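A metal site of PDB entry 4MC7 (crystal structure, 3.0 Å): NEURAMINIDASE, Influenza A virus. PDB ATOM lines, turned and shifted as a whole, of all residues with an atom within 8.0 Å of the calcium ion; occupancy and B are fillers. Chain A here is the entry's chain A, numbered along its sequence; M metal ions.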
ATOM      1  N   ASN A 198      -8.912  30.447  32.505  1.00  0.00           N
ATOM      2  CA  ASN A 198      -9.720  30.945  33.624  1.00  0.00           C
ATOM      3  C   ASN A 198     -10.308  29.793  34.462  1.00  0.00           C
ATOM      4  O   ASN A 198     -10.700  28.756  33.939  1.00  0.00           O
ATOM      5  CB  ASN A 198     -10.800  31.889  33.067  1.00  0.00           C
ATOM      6  CG  ASN A 198     -12.014  31.986  33.952  1.00  0.00           C
ATOM      7  OD1 ASN A 198     -13.088  31.463  33.615  1.00  0.00           O
ATOM      8  ND2 ASN A 198     -11.852  32.623  35.100  1.00  0.00           N
ATOM      9  N   THR A 216     -14.015  25.826  36.596  1.00  0.00           N
ATOM     10  CA  THR A 216     -14.938  26.093  35.509  1.00  0.00           C
ATOM     11  C   THR A 216     -14.373  27.266  34.692  1.00  0.00           C
ATOM     12  O   THR A 216     -14.101  28.353  35.199  1.00  0.00           O
ATOM     13  CB  THR A 216     -16.317  26.415  36.096  1.00  0.00           C
ATOM     14  OG1 THR A 216     -17.013  25.178  36.362  1.00  0.00           O
ATOM     15  CG2 THR A 216     -17.153  27.242  35.161  1.00  0.00           C
ATOM     16  N   ASN A 217     -14.151  27.025  33.406  1.00  0.00           N
ATOM     17  CA  ASN A 217     -13.534  28.056  32.591  1.00  0.00           C
ATOM     18  C   ASN A 217     -14.637  28.775  31.871  1.00  0.00           C
ATOM     19  O   ASN A 217     -15.297  28.207  30.958  1.00  0.00           O
ATOM     20  CB  ASN A 217     -12.552  27.434  31.609  1.00  0.00           C
ATOM     21  CG  ASN A 217     -11.787  28.457  30.806  1.00  0.00           C
ATOM     22  OD1 ASN A 217     -12.298  29.516  30.401  1.00  0.00           O
ATOM     23  ND2 ASN A 217     -10.526  28.120  30.524  1.00  0.00           N
ATOM     24  N   LEU A 218     -14.843  30.026  32.293  1.00  0.00           N
ATOM     25  CA  LEU A 218     -15.926  30.852  31.755  1.00  0.00           C
ATOM     26  C   LEU A 218     -15.510  31.620  30.523  1.00  0.00           C
ATOM     27  O   LEU A 218     -16.326  32.362  29.960  1.00  0.00           O
ATOM     28  CB  LEU A 218     -16.466  31.825  32.788  1.00  0.00           C
ATOM     29  CG  LEU A 218     -17.355  31.244  33.866  1.00  0.00           C
ATOM     30  CD1 LEU A 218     -16.483  31.023  35.045  1.00  0.00           C
ATOM     31  CD2 LEU A 218     -18.429  32.241  34.215  1.00  0.00           C
ATOM     32  N   TRP A 219     -14.269  31.416  30.106  1.00  0.00           N
ATOM     33  CA  TRP A 219     -13.691  32.166  29.016  1.00  0.00           C
ATOM     34  C   TRP A 219     -13.524  31.372  27.747  1.00  0.00           C
ATOM     35  O   TRP A 219     -14.316  31.539  26.826  1.00  0.00           O
ATOM     36  CB  TRP A 219     -12.360  32.725  29.476  1.00  0.00           C
ATOM     37  CG  TRP A 219     -11.566  33.467  28.449  1.00  0.00           C
ATOM     38  CD1 TRP A 219     -12.025  34.080  27.280  1.00  0.00           C
ATOM     39  CD2 TRP A 219     -10.135  33.739  28.488  1.00  0.00           C
ATOM     40  NE1 TRP A 219     -10.993  34.667  26.610  1.00  0.00           N
ATOM     41  CE2 TRP A 219      -9.830  34.494  27.286  1.00  0.00           C
ATOM     42  CE3 TRP A 219      -9.108  33.436  29.367  1.00  0.00           C
ATOM     43  CZ2 TRP A 219      -8.560  34.921  26.995  1.00  0.00           C
ATOM     44  CZ3 TRP A 219      -7.817  33.862  29.067  1.00  0.00           C
ATOM     45  CH2 TRP A 219      -7.556  34.585  27.896  1.00  0.00           C
ATOM     46  N   ASN A 220     -12.521  30.505  27.710  1.00  0.00           N
ATOM     47  CA  ASN A 220     -12.076  29.896  26.471  1.00  0.00           C
ATOM     48  C   ASN A 220     -12.142  28.385  26.454  1.00  0.00           C
ATOM     49  O   ASN A 220     -11.429  27.733  25.689  1.00  0.00           O
ATOM     50  CB  ASN A 220     -10.654  30.360  26.149  1.00  0.00           C
ATOM     51  CG  ASN A 220      -9.725  30.099  27.278  1.00  0.00           C
ATOM     52  OD1 ASN A 220     -10.061  29.360  28.194  1.00  0.00           O
ATOM     53  ND2 ASN A 220      -8.561  30.742  27.239  1.00  0.00           N
ATOM     54  N   ASP A 221     -13.024  27.807  27.257  1.00  0.00           N
ATOM     55  CA  ASP A 221     -13.009  26.363  27.458  1.00  0.00           C
ATOM     56  C   ASP A 221     -14.366  25.701  27.833  1.00  0.00           C
ATOM     57  O   ASP A 221     -15.126  26.162  28.707  1.00  0.00           O
ATOM     58  CB  ASP A 221     -11.903  26.022  28.485  1.00  0.00           C
ATOM     59  CG  ASP A 221     -11.526  24.536  28.513  1.00  0.00           C
ATOM     60  OD1 ASP A 221     -12.074  23.718  27.714  1.00  0.00           O
ATOM     61  OD2 ASP A 221     -10.646  24.195  29.350  1.00  0.00           O
ATOM     62  N   ALA A 222     -14.641  24.602  27.147  1.00  0.00           N
ATOM     63  CA  ALA A 222     -15.818  23.760  27.393  1.00  0.00           C
ATOM     64  C   ALA A 222     -15.494  22.500  28.198  1.00  0.00           C
ATOM     65  O   ALA A 222     -16.362  21.717  28.556  1.00  0.00           O
ATOM     66  CB  ALA A 222     -16.481  23.384  26.060  1.00  0.00           C
ATOM     67  N   LYS A 223     -14.220  22.283  28.457  1.00  0.00           N
ATOM     68  CA  LYS A 223     -13.811  21.272  29.392  1.00  0.00           C
ATOM     69  C   LYS A 223     -13.594  21.966  30.734  1.00  0.00           C
ATOM     70  O   LYS A 223     -13.823  23.175  30.870  1.00  0.00           O
ATOM     71  CB  LYS A 223     -12.514  20.668  28.932  1.00  0.00           C
ATOM     72  CG  LYS A 223     -12.549  19.978  27.569  1.00  0.00           C
ATOM     73  CD  LYS A 223     -11.203  19.237  27.392  1.00  0.00           C
ATOM     74  CE  LYS A 223     -10.941  18.704  25.997  1.00  0.00           C
ATOM     75  NZ  LYS A 223      -9.782  17.790  26.021  1.00  0.00           N
ATOM     76  N   ARG A 224     -13.157  21.211  31.733  1.00  0.00           N
ATOM     77  CA  ARG A 224     -12.939  21.800  33.055  1.00  0.00           C
ATOM     78  C   ARG A 224     -11.476  21.714  33.473  1.00  0.00           C
ATOM     79  O   ARG A 224     -10.895  20.636  33.541  1.00  0.00           O
ATOM     80  CB  ARG A 224     -13.837  21.169  34.135  1.00  0.00           C
ATOM     81  CG  ARG A 224     -15.251  20.861  33.688  1.00  0.00           C
ATOM     82  CD  ARG A 224     -16.144  20.582  34.876  1.00  0.00           C
ATOM     83  NE  ARG A 224     -16.866  21.799  35.185  1.00  0.00           N
ATOM     84  CZ  ARG A 224     -18.168  21.933  35.000  1.00  0.00           C
ATOM     85  NH1 ARG A 224     -18.888  20.902  34.537  1.00  0.00           N
ATOM     86  NH2 ARG A 224     -18.762  23.090  35.296  1.00  0.00           N
ATOM     87  N   PRO A 225     -10.879  22.869  33.750  1.00  0.00           N
ATOM     88  CA  PRO A 225      -9.501  22.833  34.220  1.00  0.00           C
ATOM     89  C   PRO A 225      -9.462  21.988  35.469  1.00  0.00           C
ATOM     90  O   PRO A 225     -10.499  21.776  36.116  1.00  0.00           O
ATOM     91  CB  PRO A 225      -9.230  24.297  34.574  1.00  0.00           C
ATOM     92  CG  PRO A 225     -10.258  25.080  33.777  1.00  0.00           C
ATOM     93  CD  PRO A 225     -11.450  24.234  33.787  1.00  0.00           C
ATOM     94  N   GLY A 246     -17.375  18.547  30.186  1.00  0.00           N
ATOM     95  CA  GLY A 246     -18.010  18.801  31.482  1.00  0.00           C
ATOM     96  C   GLY A 246     -18.924  20.029  31.530  1.00  0.00           C
ATOM     97  O   GLY A 246     -20.040  19.983  32.088  1.00  0.00           O
ATOM     98  N   ASP A 247     -18.440  21.101  30.933  1.00  0.00           N
ATOM     99  CA  ASP A 247     -18.983  22.457  31.126  1.00  0.00           C
ATOM    100  C   ASP A 247     -20.335  22.618  30.453  1.00  0.00           C
ATOM    101  O   ASP A 247     -20.797  21.699  29.775  1.00  0.00           O
ATOM    102  CB  ASP A 247     -17.996  23.516  30.573  1.00  0.00           C
ATOM    103  CG  ASP A 247     -17.939  24.774  31.439  1.00  0.00           C
ATOM    104  OD1 ASP A 247     -18.959  25.098  32.099  1.00  0.00           O
ATOM    105  OD2 ASP A 247     -16.848  25.445  31.440  1.00  0.00           O
ATOM    106  N   THR A 248     -20.951  23.788  30.655  1.00  0.00           N
ATOM    107  CA  THR A 248     -22.257  24.129  30.085  1.00  0.00           C
ATOM    108  C   THR A 248     -22.407  25.658  29.973  1.00  0.00           C
ATOM    109  O   THR A 248     -22.235  26.366  30.964  1.00  0.00           O
ATOM    110  CB  THR A 248     -23.404  23.583  30.928  1.00  0.00           C
ATOM    111  OG1 THR A 248     -23.329  22.144  30.998  1.00  0.00           O
ATOM    112  CG2 THR A 248     -24.760  24.019  30.348  1.00  0.00           C
ATOM    113  N   PRO A 249     -22.747  26.165  28.771  1.00  0.00           N
ATOM    114  CA  PRO A 249     -23.046  25.347  27.611  1.00  0.00           C
ATOM    115  C   PRO A 249     -21.775  24.811  26.984  1.00  0.00           C
ATOM    116  O   PRO A 249     -20.664  25.137  27.442  1.00  0.00           O
ATOM    117  CB  PRO A 249     -23.751  26.317  26.673  1.00  0.00           C
ATOM    118  CG  PRO A 249     -23.156  27.651  26.995  1.00  0.00           C
ATOM    119  CD  PRO A 249     -22.789  27.611  28.457  1.00  0.00           C
ATOM    120  N   ARG A 250     -21.965  24.007  25.938  1.00  0.00           N
ATOM    121  CA  ARG A 250     -20.897  23.292  25.227  1.00  0.00           C
ATOM    122  C   ARG A 250     -21.435  22.880  23.872  1.00  0.00           C
ATOM    123  O   ARG A 250     -22.632  22.875  23.654  1.00  0.00           O
ATOM    124  CB  ARG A 250     -20.445  22.060  25.991  1.00  0.00           C
ATOM    125  CG  ARG A 250     -21.608  21.196  26.455  1.00  0.00           C
ATOM    126  CD  ARG A 250     -21.130  19.892  27.033  1.00  0.00           C
ATOM    127  NE  ARG A 250     -22.088  19.319  27.980  1.00  0.00           N
ATOM    128  CZ  ARG A 250     -23.062  18.473  27.647  1.00  0.00           C
ATOM    129  NH1 ARG A 250     -23.214  18.096  26.392  1.00  0.00           N
ATOM    130  NH2 ARG A 250     -23.863  17.999  28.582  1.00  0.00           N
ATOM    131  N   THR A 261     -10.760  22.619  24.649  1.00  0.00           N
ATOM    132  CA  THR A 261     -11.825  22.789  23.651  1.00  0.00           C
ATOM    133  C   THR A 261     -12.423  24.180  23.578  1.00  0.00           C
ATOM    134  O   THR A 261     -13.287  24.525  24.368  1.00  0.00           O
ATOM    135  CB  THR A 261     -12.969  21.808  23.922  1.00  0.00           C
ATOM    136  OG1 THR A 261     -12.460  20.473  23.917  1.00  0.00           O
ATOM    137  CG2 THR A 261     -14.066  21.956  22.867  1.00  0.00           C
ATOM    138  N   THR A 262     -12.012  24.981  22.608  1.00  0.00           N
ATOM    139  CA  THR A 262     -12.379  26.403  22.626  1.00  0.00           C
ATOM    140  C   THR A 262     -13.773  26.683  22.082  1.00  0.00           C
ATOM    141  O   THR A 262     -14.242  27.805  22.174  1.00  0.00           O
ATOM    142  CB  THR A 262     -11.371  27.271  21.855  1.00  0.00           C
ATOM    143  OG1 THR A 262     -11.680  27.177  20.451  1.00  0.00           O
ATOM    144  CG2 THR A 262      -9.942  26.797  22.087  1.00  0.00           C
ATOM    145  N   THR A 263     -14.414  25.676  21.505  1.00  0.00           N
ATOM    146  CA  THR A 263     -15.694  25.880  20.837  1.00  0.00           C
ATOM    147  C   THR A 263     -16.803  25.872  21.857  1.00  0.00           C
ATOM    148  O   THR A 263     -16.955  24.912  22.605  1.00  0.00           O
ATOM    149  CB  THR A 263     -15.995  24.791  19.815  1.00  0.00           C
ATOM    150  OG1 THR A 263     -14.781  24.415  19.147  1.00  0.00           O
ATOM    151  CG2 THR A 263     -17.004  25.297  18.793  1.00  0.00           C
ATOM    152  N   GLU A 264     -17.596  26.949  21.843  1.00  0.00           N
ATOM    153  CA  GLU A 264     -18.597  27.242  22.873  1.00  0.00           C
ATOM    154  C   GLU A 264     -17.983  27.266  24.282  1.00  0.00           C
ATOM    155  O   GLU A 264     -18.647  27.018  25.294  1.00  0.00           O
ATOM    156  CB  GLU A 264     -19.787  26.279  22.771  1.00  0.00           C
ATOM    157  CG  GLU A 264     -20.796  26.627  21.696  1.00  0.00           C
ATOM    158  CD  GLU A 264     -22.240  26.443  22.170  1.00  0.00           C
ATOM    159  OE1 GLU A 264     -22.688  27.237  23.033  1.00  0.00           O
ATOM    160  OE2 GLU A 264     -22.934  25.512  21.680  1.00  0.00           O
ATOM    161  N   GLY A 265     -16.710  27.591  24.360  1.00  0.00           N
ATOM    162  CA  GLY A 265     -16.018  27.559  25.639  1.00  0.00           C
ATOM    163  C   GLY A 265     -16.449  28.660  26.559  1.00  0.00           C
ATOM    164  O   GLY A 265     -16.157  28.607  27.744  1.00  0.00           O
ATOM    165  N   GLU A 266     -17.154  29.656  26.014  1.00  0.00           N
ATOM    166  CA  GLU A 266     -17.545  30.825  26.782  1.00  0.00           C
ATOM    167  C   GLU A 266     -18.861  30.630  27.516  1.00  0.00           C
ATOM    168  O   GLU A 266     -19.787  30.017  26.981  1.00  0.00           O
ATOM    169  CB  GLU A 266     -17.603  32.089  25.923  1.00  0.00           C
ATOM    170  CG  GLU A 266     -17.812  33.329  26.772  1.00  0.00           C
ATOM    171  CD  GLU A 266     -17.519  34.617  26.048  1.00  0.00           C
ATOM    172  OE1 GLU A 266     -17.137  34.551  24.860  1.00  0.00           O
ATOM    173  OE2 GLU A 266     -17.655  35.690  26.671  1.00  0.00           O
ATOM    174  N   GLY A 267     -18.944  31.180  28.729  1.00  0.00           N
ATOM    175  CA  GLY A 267     -20.001  30.875  29.674  1.00  0.00           C
ATOM    176  C   GLY A 267     -19.596  29.631  30.445  1.00  0.00           C
ATOM    177  O   GLY A 267     -18.562  28.989  30.174  1.00  0.00           O
ATOM    178  N   GLY A 268     -20.411  29.255  31.417  1.00  0.00           N
ATOM    179  CA  GLY A 268     -20.064  28.129  32.241  1.00  0.00           C
ATOM    180  C   GLY A 268     -20.886  28.077  33.507  1.00  0.00           C
ATOM    181  O   GLY A 268     -21.530  29.066  33.901  1.00  0.00           O
ATOM    182  N   ILE A 269     -20.897  26.917  34.142  1.00  0.00           N
ATOM    183  CA  ILE A 269     -21.489  26.815  35.432  1.00  0.00           C
ATOM    184  C   ILE A 269     -20.676  25.836  36.264  1.00  0.00           C
ATOM    185  O   ILE A 269     -20.053  24.956  35.683  1.00  0.00           O
ATOM    186  CB  ILE A 269     -22.896  26.370  35.309  1.00  0.00           C
ATOM    187  CG1 ILE A 269     -23.677  26.636  36.621  1.00  0.00           C
ATOM    188  CG2 ILE A 269     -22.860  24.965  34.838  1.00  0.00           C
ATOM    189  CD1 ILE A 269     -25.211  26.637  36.485  1.00  0.00           C
HETATM  190 CA    CA M   1     -17.178  27.311  29.371  1.00  0.00          CA
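O of Asp 247 lies within hydrogen-bond range of NE of Arg 250.
The side-chain carboxylate (OD1) of Asp 247 lies within salt-bridge range of the guanidinium group (NH2) of Arg 224, 3.8 Å away.
The side-chain amide nitrogen of Asn 217 is in hydrogen-bond range of the side-chain amide oxygen of Asn 220 (2.7 Å).
N of Trp 219 lies within hydrogen-bond range of OD1 of Asn 217.
The side-chain carboxylate of Asp 221 sits at hydrogen-bond distance from the backbone NH of Lys 223, at 2.7 Å.
The backbone NH of Asp 247 lies close to the backbone carbonyl oxygen of Ala 222 (3.2 Å).
OD1 of Asp 247 lies within hydrogen-bond range of N of Ile 269 (3.4 Å).
ND2 of Asn 217 lies close to N of Asn 198, at 3.5 Å.
Of the 25 residues printed, 5 come within 4 Å of the calcium ion.
The calcium ion is bound by the backbone carbonyl oxygen of Gly 265 (2.3 Å), the backbone carbonyl oxygen of Gly 267 (2.3 Å), the backbone carbonyl oxygen of Asp 221 (2.4 Å), the backbone carbonyl oxygen of Asn 217 (2.6 Å) and the side-chain carboxylate of Asp 247 (2.8 Å).
The calcium ion has five donor atoms within binding distance.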
